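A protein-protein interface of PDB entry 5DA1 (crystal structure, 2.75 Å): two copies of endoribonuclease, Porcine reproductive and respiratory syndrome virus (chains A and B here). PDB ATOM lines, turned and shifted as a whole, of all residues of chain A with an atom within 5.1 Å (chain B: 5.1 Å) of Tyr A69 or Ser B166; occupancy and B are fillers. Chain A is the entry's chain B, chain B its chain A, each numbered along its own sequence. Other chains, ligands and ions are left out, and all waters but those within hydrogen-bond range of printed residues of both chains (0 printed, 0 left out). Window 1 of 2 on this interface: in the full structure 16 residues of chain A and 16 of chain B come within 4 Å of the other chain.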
ATOM      1  N   SER A   3       0.377  -1.280  -9.408  1.00  0.00           N
ATOM      2  CA  SER A   3      -0.878  -1.167 -10.141  1.00  0.00           C
ATOM      3  C   SER A   3      -1.757  -2.412  -9.888  1.00  0.00           C
ATOM      4  O   SER A   3      -1.300  -3.419  -9.291  1.00  0.00           O
ATOM      5  CB  SER A   3      -0.611  -0.954 -11.637  1.00  0.00           C
ATOM      6  OG  SER A   3       0.269  -1.929 -12.152  1.00  0.00           O
ATOM      7  N   SER A   4      -3.010  -2.337 -10.343  1.00  0.00           N
ATOM      8  CA  SER A   4      -3.988  -3.377 -10.078  1.00  0.00           C
ATOM      9  C   SER A   4      -5.089  -3.429 -11.124  1.00  0.00           C
ATOM     10  O   SER A   4      -5.415  -2.413 -11.773  1.00  0.00           O
ATOM     11  CB  SER A   4      -4.609  -3.179  -8.695  1.00  0.00           C
ATOM     12  OG  SER A   4      -5.252  -1.928  -8.580  1.00  0.00           O
ATOM     13  N   PRO A   5      -5.684  -4.614 -11.290  1.00  0.00           N
ATOM     14  CA  PRO A   5      -6.679  -4.810 -12.361  1.00  0.00           C
ATOM     15  C   PRO A   5      -7.909  -3.923 -12.243  1.00  0.00           C
ATOM     16  O   PRO A   5      -8.221  -3.407 -11.173  1.00  0.00           O
ATOM     17  CB  PRO A   5      -7.109  -6.267 -12.181  1.00  0.00           C
ATOM     18  CG  PRO A   5      -6.646  -6.629 -10.738  1.00  0.00           C
ATOM     19  CD  PRO A   5      -5.401  -5.861 -10.555  1.00  0.00           C
ATOM     20  N   LEU A   6      -8.599  -3.750 -13.362  1.00  0.00           N
ATOM     21  CA  LEU A   6      -9.927  -3.212 -13.320  1.00  0.00           C
ATOM     22  C   LEU A   6     -10.796  -4.306 -12.669  1.00  0.00           C
ATOM     23  O   LEU A   6     -10.462  -5.512 -12.745  1.00  0.00           O
ATOM     24  CB  LEU A   6     -10.381  -2.908 -14.733  1.00  0.00           C
ATOM     25  CG  LEU A   6      -9.518  -1.879 -15.489  1.00  0.00           C
ATOM     26  CD1 LEU A   6      -9.606  -2.059 -17.034  1.00  0.00           C
ATOM     27  CD2 LEU A   6      -9.894  -0.455 -15.091  1.00  0.00           C
ATOM     28  N   ALA A  67      -3.085  -3.815 -20.557  1.00  0.00           N
ATOM     29  CA  ALA A  67      -4.388  -3.651 -19.866  1.00  0.00           C
ATOM     30  C   ALA A  67      -4.664  -2.251 -19.327  1.00  0.00           C
ATOM     31  O   ALA A  67      -3.752  -1.443 -19.114  1.00  0.00           O
ATOM     32  CB  ALA A  67      -4.542  -4.657 -18.764  1.00  0.00           C
ATOM     33  N   GLY A  68      -5.943  -1.959 -19.166  1.00  0.00           N
ATOM     34  CA  GLY A  68      -6.383  -0.883 -18.294  1.00  0.00           C
ATOM     35  C   GLY A  68      -6.012  -1.252 -16.866  1.00  0.00           C
ATOM     36  O   GLY A  68      -6.043  -2.427 -16.468  1.00  0.00           O
ATOM     37  N   TYR A  69      -5.625  -0.255 -16.086  1.00  0.00           N
ATOM     38  CA  TYR A  69      -5.316  -0.531 -14.717  1.00  0.00           C
ATOM     39  C   TYR A  69      -5.657   0.619 -13.795  1.00  0.00           C
ATOM     40  O   TYR A  69      -6.019   1.709 -14.248  1.00  0.00           O
ATOM     41  CB  TYR A  69      -3.861  -0.922 -14.587  1.00  0.00           C
ATOM     42  CG  TYR A  69      -2.869   0.142 -14.973  1.00  0.00           C
ATOM     43  CD1 TYR A  69      -2.513   0.356 -16.310  1.00  0.00           C
ATOM     44  CD2 TYR A  69      -2.203   0.876 -13.994  1.00  0.00           C
ATOM     45  CE1 TYR A  69      -1.523   1.322 -16.661  1.00  0.00           C
ATOM     46  CE2 TYR A  69      -1.219   1.829 -14.327  1.00  0.00           C
ATOM     47  CZ  TYR A  69      -0.888   2.051 -15.660  1.00  0.00           C
ATOM     48  OH  TYR A  69       0.059   3.015 -15.975  1.00  0.00           O
ATOM     49  N   MET A  70      -5.513   0.352 -12.498  1.00  0.00           N
ATOM     50  CA  MET A  70      -5.777   1.336 -11.460  1.00  0.00           C
ATOM     51  C   MET A  70      -4.696   1.366 -10.458  1.00  0.00           C
ATOM     52  O   MET A  70      -4.093   0.347 -10.163  1.00  0.00           O
ATOM     53  CB  MET A  70      -7.052   1.001 -10.741  1.00  0.00           C
ATOM     54  CG  MET A  70      -8.196   1.036 -11.686  1.00  0.00           C
ATOM     55  SD  MET A  70      -9.592   1.200 -10.666  1.00  0.00           S
ATOM     56  CE  MET A  70      -9.458   2.949 -10.295  1.00  0.00           C
ATOM     57  N   VAL A  71      -4.467   2.567  -9.951  1.00  0.00           N
ATOM     58  CA  VAL A  71      -3.547   2.865  -8.859  1.00  0.00           C
ATOM     59  C   VAL A  71      -4.299   3.799  -7.921  1.00  0.00           C
ATOM     60  O   VAL A  71      -4.717   4.894  -8.319  1.00  0.00           O
ATOM     61  CB  VAL A  71      -2.303   3.593  -9.385  1.00  0.00           C
ATOM     62  CG1 VAL A  71      -1.301   3.806  -8.266  1.00  0.00           C
ATOM     63  CG2 VAL A  71      -1.677   2.823 -10.586  1.00  0.00           C
ATOM     64  N   SER A  74      -7.298   6.139  -9.037  1.00  0.00           N
ATOM     65  CA  SER A  74      -7.175   6.585 -10.416  1.00  0.00           C
ATOM     66  C   SER A  74      -7.145   5.458 -11.421  1.00  0.00           C
ATOM     67  O   SER A  74      -6.606   4.392 -11.154  1.00  0.00           O
ATOM     68  CB  SER A  74      -5.885   7.346 -10.591  1.00  0.00           C
ATOM     69  OG  SER A  74      -5.860   8.451  -9.745  1.00  0.00           O
ATOM     70  N   VAL A  75      -7.694   5.712 -12.607  1.00  0.00           N
ATOM     71  CA  VAL A  75      -7.697   4.711 -13.667  1.00  0.00           C
ATOM     72  C   VAL A  75      -6.711   5.118 -14.689  1.00  0.00           C
ATOM     73  O   VAL A  75      -6.588   6.295 -14.986  1.00  0.00           O
ATOM     74  CB  VAL A  75      -9.000   4.641 -14.396  1.00  0.00           C
ATOM     75  CG1 VAL A  75      -9.312   3.226 -14.622  1.00  0.00           C
ATOM     76  CG2 VAL A  75     -10.103   5.259 -13.584  1.00  0.00           C
ATOM     77  N   PHE A  76      -6.030   4.142 -15.263  1.00  0.00           N
ATOM     78  CA  PHE A  76      -5.046   4.434 -16.307  1.00  0.00           C
ATOM     79  C   PHE A  76      -5.270   3.608 -17.541  1.00  0.00           C
ATOM     80  O   PHE A  76      -5.773   2.491 -17.448  1.00  0.00           O
ATOM     81  CB  PHE A  76      -3.648   4.136 -15.796  1.00  0.00           C
ATOM     82  CG  PHE A  76      -3.155   5.131 -14.837  1.00  0.00           C
ATOM     83  CD1 PHE A  76      -3.545   5.077 -13.508  1.00  0.00           C
ATOM     84  CD2 PHE A  76      -2.289   6.151 -15.264  1.00  0.00           C
ATOM     85  CE1 PHE A  76      -3.056   6.025 -12.602  1.00  0.00           C
ATOM     86  CE2 PHE A  76      -1.809   7.103 -14.378  1.00  0.00           C
ATOM     87  CZ  PHE A  76      -2.191   7.043 -13.049  1.00  0.00           C
ATOM     88  N   LEU A  77      -4.871   4.156 -18.680  1.00  0.00           N
ATOM     89  CA  LEU A  77      -4.807   3.392 -19.924  1.00  0.00           C
ATOM     90  C   LEU A  77      -3.598   2.460 -19.976  1.00  0.00           C
ATOM     91  O   LEU A  77      -2.490   2.783 -19.501  1.00  0.00           O
ATOM     92  CB  LEU A  77      -4.826   4.313 -21.154  1.00  0.00           C
ATOM     93  CG  LEU A  77      -6.039   5.264 -21.240  1.00  0.00           C
ATOM     94  CD1 LEU A  77      -5.838   6.294 -22.294  1.00  0.00           C
ATOM     95  CD2 LEU A  77      -7.344   4.527 -21.521  1.00  0.00           C
ATOM     96  N   GLY A  78      -3.839   1.280 -20.537  1.00  0.00           N
ATOM     97  CA  GLY A  78      -2.777   0.414 -21.030  1.00  0.00           C
ATOM     98  C   GLY A  78      -1.947   1.084 -22.102  1.00  0.00           C
ATOM     99  O   GLY A  78      -2.450   1.843 -22.943  1.00  0.00           O
ATOM    100  N   SER A  84       1.084  -3.906 -17.702  1.00  0.00           N
ATOM    101  CA  SER A  84       0.295  -3.103 -16.769  1.00  0.00           C
ATOM    102  C   SER A  84       0.573  -3.503 -15.323  1.00  0.00           C
ATOM    103  O   SER A  84       0.981  -2.655 -14.502  1.00  0.00           O
ATOM    104  CB  SER A  84      -1.193  -3.181 -17.099  1.00  0.00           C
ATOM    105  OG  SER A  84      -1.406  -2.796 -18.455  1.00  0.00           O
ATOM    106  N   TYR A  85       0.387  -4.791 -15.029  1.00  0.00           N
ATOM    107  CA  TYR A  85       0.649  -5.361 -13.716  1.00  0.00           C
ATOM    108  C   TYR A  85       0.854  -6.836 -13.940  1.00  0.00           C
ATOM    109  O   TYR A  85       0.452  -7.364 -14.973  1.00  0.00           O
ATOM    110  CB  TYR A  85      -0.546  -5.176 -12.773  1.00  0.00           C
ATOM    111  CG  TYR A  85      -1.885  -5.471 -13.430  1.00  0.00           C
ATOM    112  CD1 TYR A  85      -2.583  -4.463 -14.089  1.00  0.00           C
ATOM    113  CD2 TYR A  85      -2.451  -6.760 -13.407  1.00  0.00           C
ATOM    114  CE1 TYR A  85      -3.783  -4.709 -14.688  1.00  0.00           C
ATOM    115  CE2 TYR A  85      -3.693  -7.015 -14.025  1.00  0.00           C
ATOM    116  CZ  TYR A  85      -4.349  -5.972 -14.666  1.00  0.00           C
ATOM    117  OH  TYR A  85      -5.563  -6.148 -15.300  1.00  0.00           O
ATOM    118  N   VAL B 140       7.198   5.591  -7.320  1.00  0.00           N
ATOM    119  CA  VAL B 140       7.224   6.969  -7.824  1.00  0.00           C
ATOM    120  C   VAL B 140       6.992   7.922  -6.675  1.00  0.00           C
ATOM    121  O   VAL B 140       6.192   7.659  -5.801  1.00  0.00           O
ATOM    122  CB  VAL B 140       6.047   7.247  -8.778  1.00  0.00           C
ATOM    123  CG1 VAL B 140       5.814   8.742  -8.930  1.00  0.00           C
ATOM    124  CG2 VAL B 140       6.259   6.612 -10.124  1.00  0.00           C
ATOM    125  N   TYR B 150       3.628  11.182 -14.530  1.00  0.00           N
ATOM    126  CA  TYR B 150       2.886  10.037 -13.978  1.00  0.00           C
ATOM    127  C   TYR B 150       1.435  10.307 -13.591  1.00  0.00           C
ATOM    128  O   TYR B 150       0.796   9.458 -12.957  1.00  0.00           O
ATOM    129  CB  TYR B 150       3.648   9.417 -12.797  1.00  0.00           C
ATOM    130  CG  TYR B 150       5.156   9.351 -13.021  1.00  0.00           C
ATOM    131  CD1 TYR B 150       5.688   8.619 -14.090  1.00  0.00           C
ATOM    132  CD2 TYR B 150       6.045  10.059 -12.193  1.00  0.00           C
ATOM    133  CE1 TYR B 150       7.070   8.575 -14.319  1.00  0.00           C
ATOM    134  CE2 TYR B 150       7.412  10.020 -12.404  1.00  0.00           C
ATOM    135  CZ  TYR B 150       7.937   9.271 -13.468  1.00  0.00           C
ATOM    136  OH  TYR B 150       9.320   9.192 -13.694  1.00  0.00           O
ATOM    137  N   LEU B 151       0.901  11.462 -13.995  1.00  0.00           N
ATOM    138  CA  LEU B 151      -0.452  11.869 -13.601  1.00  0.00           C
ATOM    139  C   LEU B 151      -1.525  11.126 -14.364  1.00  0.00           C
ATOM    140  O   LEU B 151      -1.376  10.819 -15.536  1.00  0.00           O
ATOM    141  CB  LEU B 151      -0.662  13.374 -13.781  1.00  0.00           C
ATOM    142  CG  LEU B 151       0.154  14.176 -12.784  1.00  0.00           C
ATOM    143  CD1 LEU B 151      -0.132  15.675 -12.848  1.00  0.00           C
ATOM    144  CD2 LEU B 151      -0.024  13.598 -11.381  1.00  0.00           C
ATOM    145  N   GLY B 164      -4.018   8.443  -7.575  1.00  0.00           N
ATOM    146  CA  GLY B 164      -3.037   7.398  -7.733  1.00  0.00           C
ATOM    147  C   GLY B 164      -2.114   7.866  -8.835  1.00  0.00           C
ATOM    148  O   GLY B 164      -2.510   8.700  -9.649  1.00  0.00           O
ATOM    149  N   VAL B 165      -0.889   7.340  -8.885  1.00  0.00           N
ATOM    150  CA  VAL B 165       0.106   7.868  -9.826  1.00  0.00           C
ATOM    151  C   VAL B 165       0.963   6.753 -10.513  1.00  0.00           C
ATOM    152  O   VAL B 165       1.167   5.687  -9.924  1.00  0.00           O
ATOM    153  CB  VAL B 165       0.879   8.931  -9.091  1.00  0.00           C
ATOM    154  CG1 VAL B 165       2.292   8.536  -8.903  1.00  0.00           C
ATOM    155  CG2 VAL B 165       0.703  10.256  -9.742  1.00  0.00           C
ATOM    156  N   SER B 166       1.403   6.935 -11.757  1.00  0.00           N
ATOM    157  CA  SER B 166       1.975   5.773 -12.477  1.00  0.00           C
ATOM    158  C   SER B 166       3.050   6.017 -13.499  1.00  0.00           C
ATOM    159  O   SER B 166       2.951   6.924 -14.348  1.00  0.00           O
ATOM    160  CB  SER B 166       0.900   4.950 -13.198  1.00  0.00           C
ATOM    161  OG  SER B 166       1.515   3.953 -14.023  1.00  0.00           O
ATOM    162  N   SER B 167       4.054   5.149 -13.415  1.00  0.00           N
ATOM    163  CA  SER B 167       5.093   5.019 -14.440  1.00  0.00           C
ATOM    164  C   SER B 167       4.851   3.682 -15.071  1.00  0.00           C
ATOM    165  O   SER B 167       5.262   2.647 -14.529  1.00  0.00           O
ATOM    166  CB  SER B 167       6.492   5.061 -13.837  1.00  0.00           C
ATOM    167  OG  SER B 167       7.452   5.056 -14.864  1.00  0.00           O
ATOM    168  N   PRO B 168       4.157   3.686 -16.209  1.00  0.00           N
ATOM    169  CA  PRO B 168       3.602   2.457 -16.774  1.00  0.00           C
ATOM    170  C   PRO B 168       4.680   1.402 -16.925  1.00  0.00           C
ATOM    171  O   PRO B 168       5.688   1.621 -17.593  1.00  0.00           O
ATOM    172  CB  PRO B 168       3.092   2.884 -18.157  1.00  0.00           C
ATOM    173  CG  PRO B 168       3.208   4.361 -18.215  1.00  0.00           C
ATOM    174  CD  PRO B 168       4.154   4.803 -17.163  1.00  0.00           C
ATOM    175  N   ALA B 171       6.637   1.711 -12.005  1.00  0.00           N
ATOM    176  CA  ALA B 171       6.247   2.081 -10.650  1.00  0.00           C
ATOM    177  C   ALA B 171       4.758   2.507 -10.509  1.00  0.00           C
ATOM    178  O   ALA B 171       4.075   2.767 -11.523  1.00  0.00           O
ATOM    179  CB  ALA B 171       7.178   3.158 -10.160  1.00  0.00           C
ATOM    180  N   ALA B 172       4.269   2.568  -9.263  1.00  0.00           N
ATOM    181  CA  ALA B 172       2.915   3.062  -8.951  1.00  0.00           C
ATOM    182  C   ALA B 172       2.810   3.570  -7.503  1.00  0.00           C
ATOM    183  O   ALA B 172       3.520   3.043  -6.624  1.00  0.00           O
ATOM    184  CB  ALA B 172       1.908   1.965  -9.157  1.00  0.00           C
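The side-chain hydroxyl (OG) of Ser B166 sits at hydrogen-bond distance from the side-chain hydroxyl (OH) of Tyr A69, at 2.6 Å. The side-chain hydroxyl (OG) of Ser A74 lies within hydrogen-bond range of the backbone NH (N) of Gly B164 (2.8 Å).
The backbone NH (N) of Ser B166 lies within hydrogen-bond range of the backbone carbonyl oxygen (O) of Tyr B150 (2.9 Å). OG of Ser A3 lies within hydrogen-bond range of O of Ser A84, at 2.6 Å. O of Tyr A69 sits at hydrogen-bond distance from N of Phe A76 (2.6 Å).
N of Ser A3 touches CB of Ala B172 (3.6 Å). Tyr A69 touches Pro B168 (OH to CA, 3.7 Å). Val A71 touches Gly B164 (O to CA, 3.1 Å). Val A71 touches Val B165 (CG1 to O, 3.5 Å). Ala B172 touches Val A71 (CB to CG1, 3.8 Å). Tyr B150 touches Phe A76. Phe A76 touches Leu B151 (CE2 to O, 3.9 Å). Phe A76 touches Gly B164 (CZ to O, 3.8 Å). Phe A76 touches Ser B166.
Tyr A69 touches just these residues of chain B: Ser B166 (2.6 Å) and Pro B168 (3.7 Å). Printed residues of chain A within 4 Å of Ser B166: Tyr A69 (2.6 Å) and Phe A76 (3.7 Å). Of the printed residues of chain B, Phe A76 touches Tyr B150 (3.8 Å), Leu B151 (3.9 Å), Gly B164 (3.8 Å) and Ser B166 (3.7 Å). Printed residues of chain A within 4 Å of Tyr B150: Phe A76 (3.8 Å). Gly A68 touches none of the printed residues of chain B. Ser A4 touches none of the printed residues of chain B. The nearest printed residue of chain B that does not touch Val A71 is Ser B166 (4.2 Å).
Printed residues of chain B that touch a printed residue of chain A: Tyr B150, Leu B151, Gly B164, Val B165, Ser B166, Pro B168 and Ala B172. Hydrophobic or aromatic side chains of chain B within 4 Å of the printed part of chain A: Pro B168 and Ala B172.
No position is printed for both chains. Of the 11 pairs that touch across the chains among the printed residues, none has its exchanged pair printed and touching as well.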
